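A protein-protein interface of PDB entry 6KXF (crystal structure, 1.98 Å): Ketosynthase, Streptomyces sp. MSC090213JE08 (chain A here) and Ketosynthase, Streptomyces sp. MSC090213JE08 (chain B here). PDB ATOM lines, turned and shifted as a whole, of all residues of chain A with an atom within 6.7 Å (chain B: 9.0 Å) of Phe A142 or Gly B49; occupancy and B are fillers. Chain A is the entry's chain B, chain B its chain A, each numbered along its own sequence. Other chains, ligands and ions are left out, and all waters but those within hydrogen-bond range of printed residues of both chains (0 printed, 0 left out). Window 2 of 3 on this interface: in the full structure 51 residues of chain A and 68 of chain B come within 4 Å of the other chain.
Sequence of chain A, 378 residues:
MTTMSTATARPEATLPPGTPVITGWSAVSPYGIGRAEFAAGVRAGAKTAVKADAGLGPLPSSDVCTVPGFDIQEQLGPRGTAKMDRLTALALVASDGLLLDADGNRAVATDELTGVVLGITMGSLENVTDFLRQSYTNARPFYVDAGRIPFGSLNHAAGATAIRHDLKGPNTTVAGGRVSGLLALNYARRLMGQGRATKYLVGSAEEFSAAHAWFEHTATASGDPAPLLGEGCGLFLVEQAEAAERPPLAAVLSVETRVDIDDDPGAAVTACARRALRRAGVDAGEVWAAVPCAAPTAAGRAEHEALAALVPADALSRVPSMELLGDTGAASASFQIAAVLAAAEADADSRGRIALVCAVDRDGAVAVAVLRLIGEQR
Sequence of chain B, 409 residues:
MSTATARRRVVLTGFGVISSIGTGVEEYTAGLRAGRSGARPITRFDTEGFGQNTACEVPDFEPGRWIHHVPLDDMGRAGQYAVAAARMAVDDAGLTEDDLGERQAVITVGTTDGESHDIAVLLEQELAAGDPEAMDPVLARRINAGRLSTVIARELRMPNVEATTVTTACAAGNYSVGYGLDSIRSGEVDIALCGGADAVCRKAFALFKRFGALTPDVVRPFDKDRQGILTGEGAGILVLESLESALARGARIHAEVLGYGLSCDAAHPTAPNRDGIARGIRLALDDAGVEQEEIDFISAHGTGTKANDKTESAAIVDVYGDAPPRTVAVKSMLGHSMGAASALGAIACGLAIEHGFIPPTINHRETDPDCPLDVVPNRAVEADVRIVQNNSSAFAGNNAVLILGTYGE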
ATOM      1  N   GLN A 134     -23.150  14.233 -16.000  1.00  0.00           N
ATOM      2  CA  GLN A 134     -23.099  14.990 -17.234  1.00  0.00           C
ATOM      3  C   GLN A 134     -21.917  15.974 -17.189  1.00  0.00           C
ATOM      4  O   GLN A 134     -21.262  16.193 -18.239  1.00  0.00           O
ATOM      5  CB  GLN A 134     -24.496  15.485 -17.644  1.00  0.00           C
ATOM      6  CG  GLN A 134     -25.154  16.518 -16.764  1.00  0.00           C
ATOM      7  CD  GLN A 134     -26.609  16.747 -17.127  1.00  0.00           C
ATOM      8  OE1 GLN A 134     -27.430  17.069 -16.274  1.00  0.00           O
ATOM      9  NE2 GLN A 134     -26.959  16.635 -18.400  1.00  0.00           N
ATOM     10  N   SER A 135     -21.551  16.472 -15.996  1.00  0.00           N
ATOM     11  CA  SER A 135     -20.370  17.340 -15.868  1.00  0.00           C
ATOM     12  C   SER A 135     -19.111  16.610 -16.334  1.00  0.00           C
ATOM     13  O   SER A 135     -18.238  17.214 -16.922  1.00  0.00           O
ATOM     14  CB  SER A 135     -20.142  17.834 -14.452  1.00  0.00           C
ATOM     15  OG  SER A 135     -18.988  18.656 -14.435  1.00  0.00           O
ATOM     16  N   ALA A 139     -19.299  17.526 -23.163  1.00  0.00           N
ATOM     17  CA  ALA A 139     -18.127  18.053 -23.879  1.00  0.00           C
ATOM     18  C   ALA A 139     -17.497  19.196 -23.082  1.00  0.00           C
ATOM     19  O   ALA A 139     -16.314  19.452 -23.221  1.00  0.00           O
ATOM     20  CB  ALA A 139     -18.500  18.505 -25.276  1.00  0.00           C
ATOM     21  N   ARG A 140     -18.305  19.902 -22.287  1.00  0.00           N
ATOM     22  CA  ARG A 140     -17.784  20.912 -21.355  1.00  0.00           C
ATOM     23  C   ARG A 140     -18.372  20.596 -19.993  1.00  0.00           C
ATOM     24  O   ARG A 140     -19.517  20.165 -19.927  1.00  0.00           O
ATOM     25  CB  ARG A 140     -18.144  22.342 -21.778  1.00  0.00           C
ATOM     26  CG  ARG A 140     -17.463  22.791 -23.065  1.00  0.00           C
ATOM     27  CD  ARG A 140     -17.929  24.171 -23.477  1.00  0.00           C
ATOM     28  NE  ARG A 140     -17.897  24.364 -24.919  1.00  0.00           N
ATOM     29  CZ  ARG A 140     -16.789  24.583 -25.604  1.00  0.00           C
ATOM     30  NH1 ARG A 140     -15.635  24.677 -24.965  1.00  0.00           N
ATOM     31  NH2 ARG A 140     -16.839  24.691 -26.918  1.00  0.00           N
ATOM     32  N   PRO A 141     -17.616  20.788 -18.892  1.00  0.00           N
ATOM     33  CA  PRO A 141     -18.035  20.267 -17.593  1.00  0.00           C
ATOM     34  C   PRO A 141     -19.166  21.087 -16.940  1.00  0.00           C
ATOM     35  O   PRO A 141     -19.657  20.689 -15.886  1.00  0.00           O
ATOM     36  CB  PRO A 141     -16.703  20.240 -16.826  1.00  0.00           C
ATOM     37  CG  PRO A 141     -15.916  21.401 -17.377  1.00  0.00           C
ATOM     38  CD  PRO A 141     -16.337  21.516 -18.828  1.00  0.00           C
ATOM     39  N   PHE A 142     -19.594  22.182 -17.587  1.00  0.00           N
ATOM     40  CA  PHE A 142     -20.735  22.966 -17.171  1.00  0.00           C
ATOM     41  C   PHE A 142     -21.953  22.733 -18.088  1.00  0.00           C
ATOM     42  O   PHE A 142     -23.012  23.405 -17.923  1.00  0.00           O
ATOM     43  CB  PHE A 142     -20.373  24.451 -17.036  1.00  0.00           C
ATOM     44  CG  PHE A 142     -19.952  25.161 -18.296  1.00  0.00           C
ATOM     45  CD1 PHE A 142     -18.616  25.270 -18.620  1.00  0.00           C
ATOM     46  CD2 PHE A 142     -20.887  25.778 -19.109  1.00  0.00           C
ATOM     47  CE1 PHE A 142     -18.221  25.909 -19.781  1.00  0.00           C
ATOM     48  CE2 PHE A 142     -20.491  26.437 -20.264  1.00  0.00           C
ATOM     49  CZ  PHE A 142     -19.160  26.491 -20.602  1.00  0.00           C
ATOM     50  N   TYR A 143     -21.844  21.778 -19.022  1.00  0.00           N
ATOM     51  CA  TYR A 143     -23.023  21.274 -19.771  1.00  0.00           C
ATOM     52  C   TYR A 143     -23.834  20.351 -18.866  1.00  0.00           C
ATOM     53  O   TYR A 143     -23.761  19.129 -18.995  1.00  0.00           O
ATOM     54  CB  TYR A 143     -22.625  20.551 -21.059  1.00  0.00           C
ATOM     55  CG  TYR A 143     -22.068  21.434 -22.147  1.00  0.00           C
ATOM     56  CD1 TYR A 143     -22.029  22.815 -22.019  1.00  0.00           C
ATOM     57  CD2 TYR A 143     -21.609  20.881 -23.337  1.00  0.00           C
ATOM     58  CE1 TYR A 143     -21.510  23.612 -23.024  1.00  0.00           C
ATOM     59  CE2 TYR A 143     -21.097  21.670 -24.355  1.00  0.00           C
ATOM     60  CZ  TYR A 143     -21.051  23.044 -24.200  1.00  0.00           C
ATOM     61  OH  TYR A 143     -20.550  23.845 -25.193  1.00  0.00           O
ATOM     62  N   VAL A 144     -24.594  20.977 -17.960  1.00  0.00           N
ATOM     63  CA  VAL A 144     -25.450  20.298 -17.018  1.00  0.00           C
ATOM     64  C   VAL A 144     -26.879  20.818 -17.201  1.00  0.00           C
ATOM     65  O   VAL A 144     -27.100  21.911 -17.741  1.00  0.00           O
ATOM     66  CB  VAL A 144     -24.939  20.467 -15.568  1.00  0.00           C
ATOM     67  CG1 VAL A 144     -23.526  19.925 -15.434  1.00  0.00           C
ATOM     68  CG2 VAL A 144     -25.008  21.906 -15.087  1.00  0.00           C
ATOM     69  N   ASP A 145     -27.841  20.015 -16.737  1.00  0.00           N
ATOM     70  CA  ASP A 145     -29.238  20.269 -16.949  1.00  0.00           C
ATOM     71  C   ASP A 145     -29.661  21.346 -15.958  1.00  0.00           C
ATOM     72  O   ASP A 145     -29.861  21.046 -14.778  1.00  0.00           O
ATOM     73  CB  ASP A 145     -30.058  18.987 -16.776  1.00  0.00           C
ATOM     74  CG  ASP A 145     -31.533  19.121 -17.147  1.00  0.00           C
ATOM     75  OD1 ASP A 145     -32.083  20.242 -17.009  1.00  0.00           O
ATOM     76  OD2 ASP A 145     -32.126  18.100 -17.569  1.00  0.00           O
ATOM     77  N   ASP B  46     -10.386  19.209 -10.691  1.00  0.00           N
ATOM     78  CA  ASP B  46      -9.823  19.591 -11.974  1.00  0.00           C
ATOM     79  C   ASP B  46     -10.783  20.574 -12.638  1.00  0.00           C
ATOM     80  O   ASP B  46     -11.953  20.245 -12.852  1.00  0.00           O
ATOM     81  CB  ASP B  46      -9.577  18.369 -12.866  1.00  0.00           C
ATOM     82  CG  ASP B  46      -9.045  18.703 -14.257  1.00  0.00           C
ATOM     83  OD1 ASP B  46      -8.398  19.786 -14.418  1.00  0.00           O
ATOM     84  OD2 ASP B  46      -9.288  17.885 -15.181  1.00  0.00           O
ATOM     85  N   THR B  47     -10.290  21.791 -12.915  1.00  0.00           N
ATOM     86  CA  THR B  47     -11.101  22.846 -13.467  1.00  0.00           C
ATOM     87  C   THR B  47     -10.997  22.914 -15.008  1.00  0.00           C
ATOM     88  O   THR B  47     -11.600  23.774 -15.605  1.00  0.00           O
ATOM     89  CB  THR B  47     -10.756  24.201 -12.836  1.00  0.00           C
ATOM     90  OG1 THR B  47      -9.390  24.491 -13.087  1.00  0.00           O
ATOM     91  CG2 THR B  47     -11.011  24.256 -11.339  1.00  0.00           C
ATOM     92  N   GLU B  48     -10.232  22.029 -15.642  1.00  0.00           N
ATOM     93  CA  GLU B  48     -10.063  22.078 -17.096  1.00  0.00           C
ATOM     94  C   GLU B  48     -11.451  22.112 -17.756  1.00  0.00           C
ATOM     95  O   GLU B  48     -12.302  21.263 -17.512  1.00  0.00           O
ATOM     96  CB  GLU B  48      -9.170  20.928 -17.580  1.00  0.00           C
ATOM     97  CG  GLU B  48      -8.836  20.993 -19.061  1.00  0.00           C
ATOM     98  CD  GLU B  48      -8.067  22.238 -19.481  1.00  0.00           C
ATOM     99  OE1 GLU B  48      -8.394  22.817 -20.520  1.00  0.00           O
ATOM    100  OE2 GLU B  48      -7.137  22.625 -18.764  1.00  0.00           O
ATOM    101  N   GLY B  49     -11.687  23.145 -18.571  1.00  0.00           N
ATOM    102  CA  GLY B  49     -12.903  23.258 -19.357  1.00  0.00           C
ATOM    103  C   GLY B  49     -13.917  24.218 -18.767  1.00  0.00           C
ATOM    104  O   GLY B  49     -14.922  24.549 -19.434  1.00  0.00           O
ATOM    105  N   PHE B  50     -13.693  24.658 -17.512  1.00  0.00           N
ATOM    106  CA  PHE B  50     -14.602  25.630 -16.866  1.00  0.00           C
ATOM    107  C   PHE B  50     -14.293  27.075 -17.289  1.00  0.00           C
ATOM    108  O   PHE B  50     -15.169  27.960 -17.209  1.00  0.00           O
ATOM    109  CB  PHE B  50     -14.562  25.466 -15.342  1.00  0.00           C
ATOM    110  CG  PHE B  50     -15.356  24.298 -14.824  1.00  0.00           C
ATOM    111  CD1 PHE B  50     -16.736  24.370 -14.719  1.00  0.00           C
ATOM    112  CD2 PHE B  50     -14.724  23.149 -14.387  1.00  0.00           C
ATOM    113  CE1 PHE B  50     -17.471  23.307 -14.211  1.00  0.00           C
ATOM    114  CE2 PHE B  50     -15.456  22.094 -13.878  1.00  0.00           C
ATOM    115  CZ  PHE B  50     -16.830  22.177 -13.792  1.00  0.00           C
ATOM    116  N   GLY B  51     -13.069  27.308 -17.763  1.00  0.00           N
ATOM    117  CA  GLY B  51     -12.653  28.616 -18.242  1.00  0.00           C
ATOM    118  C   GLY B  51     -12.174  29.531 -17.128  1.00  0.00           C
ATOM    119  O   GLY B  51     -11.979  30.701 -17.391  1.00  0.00           O
ATOM    120  N   GLN B  52     -12.022  28.991 -15.902  1.00  0.00           N
ATOM    121  CA  GLN B  52     -11.556  29.722 -14.686  1.00  0.00           C
ATOM    122  C   GLN B  52     -11.191  28.704 -13.599  1.00  0.00           C
ATOM    123  O   GLN B  52     -11.607  27.511 -13.606  1.00  0.00           O
ATOM    124  CB  GLN B  52     -12.565  30.771 -14.190  1.00  0.00           C
ATOM    125  CG  GLN B  52     -13.970  30.232 -13.907  1.00  0.00           C
ATOM    126  CD  GLN B  52     -15.036  31.296 -13.727  1.00  0.00           C
ATOM    127  OE1 GLN B  52     -15.850  31.526 -14.611  1.00  0.00           O
ATOM    128  NE2 GLN B  52     -15.094  31.924 -12.557  1.00  0.00           N
ATOM    129  N   ASN B  53     -10.406  29.189 -12.646  1.00  0.00           N
ATOM    130  CA  ASN B  53      -9.637  28.351 -11.769  1.00  0.00           C
ATOM    131  C   ASN B  53      -9.530  28.910 -10.325  1.00  0.00           C
ATOM    132  O   ASN B  53      -8.686  28.458  -9.574  1.00  0.00           O
ATOM    133  CB  ASN B  53      -8.238  28.164 -12.370  1.00  0.00           C
ATOM    134  CG  ASN B  53      -7.471  27.050 -11.691  1.00  0.00           C
ATOM    135  OD1 ASN B  53      -7.993  25.945 -11.530  1.00  0.00           O
ATOM    136  ND2 ASN B  53      -6.264  27.346 -11.234  1.00  0.00           N
ATOM    137  N   ARG B 202     -16.804  20.151  -7.098  1.00  0.00           N
ATOM    138  CA  ARG B 202     -17.093  20.344  -8.477  1.00  0.00           C
ATOM    139  C   ARG B 202     -18.547  20.756  -8.653  1.00  0.00           C
ATOM    140  O   ARG B 202     -18.848  21.588  -9.492  1.00  0.00           O
ATOM    141  CB  ARG B 202     -16.808  19.054  -9.239  1.00  0.00           C
ATOM    142  CG  ARG B 202     -16.972  19.200 -10.741  1.00  0.00           C
ATOM    143  CD  ARG B 202     -16.246  18.051 -11.407  1.00  0.00           C
ATOM    144  NE  ARG B 202     -16.559  18.035 -12.811  1.00  0.00           N
ATOM    145  CZ  ARG B 202     -15.688  17.730 -13.743  1.00  0.00           C
ATOM    146  NH1 ARG B 202     -14.425  17.507 -13.417  1.00  0.00           N
ATOM    147  NH2 ARG B 202     -16.093  17.636 -14.990  1.00  0.00           N
ATOM    148  N   LYS B 203     -19.436  20.158  -7.864  1.00  0.00           N
ATOM    149  CA  LYS B 203     -20.868  20.386  -8.052  1.00  0.00           C
ATOM    150  C   LYS B 203     -21.210  21.872  -7.896  1.00  0.00           C
ATOM    151  O   LYS B 203     -21.896  22.441  -8.758  1.00  0.00           O
ATOM    152  CB  LYS B 203     -21.698  19.547  -7.080  1.00  0.00           C
ATOM    153  CG  LYS B 203     -23.213  19.716  -7.178  1.00  0.00           C
ATOM    154  CD  LYS B 203     -23.836  19.470  -5.823  1.00  0.00           C
ATOM    155  CE  LYS B 203     -25.320  19.725  -5.711  1.00  0.00           C
ATOM    156  NZ  LYS B 203     -25.718  19.496  -4.297  1.00  0.00           N
ATOM    157  N   PHE B 205     -19.293  24.521  -8.047  1.00  0.00           N
ATOM    158  CA  PHE B 205     -18.628  25.322  -9.032  1.00  0.00           C
ATOM    159  C   PHE B 205     -19.405  25.277 -10.366  1.00  0.00           C
ATOM    160  O   PHE B 205     -19.697  26.317 -10.951  1.00  0.00           O
ATOM    161  CB  PHE B 205     -17.204  24.818  -9.174  1.00  0.00           C
ATOM    162  CG  PHE B 205     -16.277  25.690  -9.969  1.00  0.00           C
ATOM    163  CD1 PHE B 205     -15.902  26.935  -9.497  1.00  0.00           C
ATOM    164  CD2 PHE B 205     -15.679  25.211 -11.125  1.00  0.00           C
ATOM    165  CE1 PHE B 205     -14.984  27.707 -10.190  1.00  0.00           C
ATOM    166  CE2 PHE B 205     -14.769  25.992 -11.827  1.00  0.00           C
ATOM    167  CZ  PHE B 205     -14.411  27.230 -11.348  1.00  0.00           C
ATOM    168  N   ALA B 206     -19.751  24.079 -10.828  1.00  0.00           N
ATOM    169  CA  ALA B 206     -20.509  23.912 -12.097  1.00  0.00           C
ATOM    170  C   ALA B 206     -21.902  24.533 -11.984  1.00  0.00           C
ATOM    171  O   ALA B 206     -22.403  25.139 -12.948  1.00  0.00           O
ATOM    172  CB  ALA B 206     -20.611  22.452 -12.435  1.00  0.00           C
ATOM    173  N   LEU B 207     -22.531  24.357 -10.816  1.00  0.00           N
ATOM    174  CA  LEU B 207     -23.859  24.893 -10.569  1.00  0.00           C
ATOM    175  C   LEU B 207     -23.845  26.404 -10.826  1.00  0.00           C
ATOM    176  O   LEU B 207     -24.654  26.943 -11.634  1.00  0.00           O
ATOM    177  CB  LEU B 207     -24.268  24.597  -9.122  1.00  0.00           C
ATOM    178  CG  LEU B 207     -25.734  24.832  -8.743  1.00  0.00           C
ATOM    179  CD1 LEU B 207     -26.092  24.030  -7.499  1.00  0.00           C
ATOM    180  CD2 LEU B 207     -26.059  26.307  -8.500  1.00  0.00           C
ATOM    181  N   PHE B 208     -22.931  27.098 -10.137  1.00  0.00           N
ATOM    182  CA  PHE B 208     -22.909  28.561 -10.231  1.00  0.00           C
ATOM    183  C   PHE B 208     -22.494  28.970 -11.638  1.00  0.00           C
ATOM    184  O   PHE B 208     -23.029  29.930 -12.167  1.00  0.00           O
ATOM    185  CB  PHE B 208     -22.061  29.187  -9.122  1.00  0.00           C
ATOM    186  CG  PHE B 208     -22.891  29.361  -7.876  1.00  0.00           C
ATOM    187  CD1 PHE B 208     -23.765  30.432  -7.760  1.00  0.00           C
ATOM    188  CD2 PHE B 208     -22.899  28.393  -6.883  1.00  0.00           C
ATOM    189  CE1 PHE B 208     -24.569  30.579  -6.639  1.00  0.00           C
ATOM    190  CE2 PHE B 208     -23.703  28.539  -5.760  1.00  0.00           C
ATOM    191  CZ  PHE B 208     -24.535  29.628  -5.643  1.00  0.00           C
ATOM    192  N   LYS B 209     -21.552  28.236 -12.230  1.00  0.00           N
ATOM    193  CA  LYS B 209     -21.170  28.494 -13.648  1.00  0.00           C
ATOM    194  C   LYS B 209     -22.424  28.439 -14.540  1.00  0.00           C
ATOM    195  O   LYS B 209     -22.768  29.409 -15.212  1.00  0.00           O
ATOM    196  CB  LYS B 209     -20.073  27.516 -14.063  1.00  0.00           C
ATOM    197  CG  LYS B 209     -19.529  27.707 -15.470  1.00  0.00           C
ATOM    198  CD  LYS B 209     -19.063  29.094 -15.805  1.00  0.00           C
ATOM    199  CE  LYS B 209     -18.768  29.208 -17.285  1.00  0.00           C
ATOM    200  NZ  LYS B 209     -17.867  30.347 -17.540  1.00  0.00           N
ATOM    201  N   ARG B 210     -23.179  27.344 -14.432  1.00  0.00           N
ATOM    202  CA  ARG B 210     -24.347  27.107 -15.291  1.00  0.00           C
ATOM    203  C   ARG B 210     -25.378  28.231 -15.105  1.00  0.00           C
ATOM    204  O   ARG B 210     -26.052  28.581 -16.076  1.00  0.00           O
ATOM    205  CB  ARG B 210     -24.977  25.729 -15.045  1.00  0.00           C
ATOM    206  CG  ARG B 210     -26.206  25.412 -15.897  1.00  0.00           C
ATOM    207  CD  ARG B 210     -25.910  25.229 -17.388  1.00  0.00           C
ATOM    208  NE  ARG B 210     -25.645  26.512 -18.039  1.00  0.00           N
ATOM    209  CZ  ARG B 210     -24.969  26.669 -19.175  1.00  0.00           C
ATOM    210  NH1 ARG B 210     -24.670  27.889 -19.615  1.00  0.00           N
ATOM    211  NH2 ARG B 210     -24.618  25.599 -19.872  1.00  0.00           N
ATOM    212  N   PHE B 211     -25.500  28.789 -13.889  1.00  0.00           N
ATOM    213  CA  PHE B 211     -26.484  29.850 -13.635  1.00  0.00           C
ATOM    214  C   PHE B 211     -25.934  31.246 -13.974  1.00  0.00           C
ATOM    215  O   PHE B 211     -26.620  32.240 -13.809  1.00  0.00           O
ATOM    216  CB  PHE B 211     -26.979  29.799 -12.188  1.00  0.00           C
ATOM    217  CG  PHE B 211     -28.169  28.913 -11.883  1.00  0.00           C
ATOM    218  CD1 PHE B 211     -28.905  28.271 -12.874  1.00  0.00           C
ATOM    219  CD2 PHE B 211     -28.590  28.767 -10.570  1.00  0.00           C
ATOM    220  CE1 PHE B 211     -30.005  27.482 -12.565  1.00  0.00           C
ATOM    221  CE2 PHE B 211     -29.692  27.984 -10.259  1.00  0.00           C
ATOM    222  CZ  PHE B 211     -30.404  27.349 -11.256  1.00  0.00           C
ATOM    223  N   GLY B 212     -24.712  31.321 -14.481  1.00  0.00           N
ATOM    224  CA  GLY B 212     -24.092  32.576 -14.806  1.00  0.00           C
ATOM    225  C   GLY B 212     -23.883  33.473 -13.589  1.00  0.00           C
ATOM    226  O   GLY B 212     -23.940  34.688 -13.740  1.00  0.00           O
ATOM    227  N   LEU B 214     -21.129  32.975 -11.295  1.00  0.00           N
ATOM    228  CA  LEU B 214     -19.746  32.836 -10.886  1.00  0.00           C
ATOM    229  C   LEU B 214     -18.966  34.019 -11.472  1.00  0.00           C
ATOM    230  O   LEU B 214     -18.957  34.188 -12.656  1.00  0.00           O
ATOM    231  CB  LEU B 214     -19.278  31.499 -11.458  1.00  0.00           C
ATOM    232  CG  LEU B 214     -18.089  30.809 -10.830  1.00  0.00           C
ATOM    233  CD1 LEU B 214     -18.339  30.499  -9.363  1.00  0.00           C
ATOM    234  CD2 LEU B 214     -17.821  29.532 -11.601  1.00  0.00           C
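Of the 19 printed residues of chain B, 7 touch a printed residue of chain A. Printed residues of chain B that touch a printed residue of chain A: Glu B48, Gly B49, Phe B50, Arg B202, Ala B206, Lys B209 and Arg B210. Hydrophobic or aromatic side chains of chain A within 4 Å of the printed part of chain B: Pro A141, Phe A142 and Val A144. Along chain A the printed residues that touch a printed residue of chain B span positions 135 to 144. Among the printed residues, 10 pairs touch across the chains. Among the printed residues, no Asp or Glu carboxylate lies within 4 Å of a Lys or Arg side-chain nitrogen of the other chain.
O of Glu B48 touches CG of Pro A141, 3.6 Å away. Pro A141 touches Gly B49. Pro A141 touches Phe B50 (CG to CE2, 3.6 Å). Pro A141 touches Arg B202. CB of Ala B206 touches O of Pro A141 (3.99 Å). Gly B49 touches Phe A142 (O to CE1, 3.6 Å). Lys B209 touches Phe A142. Val A144 touches Arg B210.
The guanidinium group (NH2) of Arg B202 lies within hydrogen-bond range of the backbone carbonyl oxygen (O) of Ser A135 (2.9 Å). NH2 of Arg B210 is in hydrogen-bond range of O of Phe A142 (3.3 Å).
The side-chain carboxylate of Asp B46 is in hydrogen-bond range of the backbone NH of Glu B48, 3.1 Å away. OG of Ser A135 is in hydrogen-bond range of O of Pro A141 (2.6 Å).
Of the printed residues of chain B, Pro A141 touches Glu B48 (3.6 Å), Gly B49 (3.4 Å), Phe B50 (3.6 Å), Arg B202 (3.2 Å) and Ala B206 (3.99 Å). Val A144 touches just one residue of chain B: Arg B210 (3.5 Å). Of the printed residues of chain A, Gly B49 touches Pro A141 (3.4 Å) and Phe A142 (3.6 Å). Of the printed residues of chain A, Phe B50 touches Pro A141. Printed residues of chain A within 4 Å of Ala B206: Pro A141 (3.99 Å). Printed residues of chain A within 4 Å of Arg B210: Phe A142 (3.3 Å) and Val A144 (3.5 Å). The nearest residue of chain B that does not touch Phe A142 is Phe B50 (4.1 Å). The nearest residue of chain A that does not touch Gly B49 is Arg A140 (4.6 Å).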
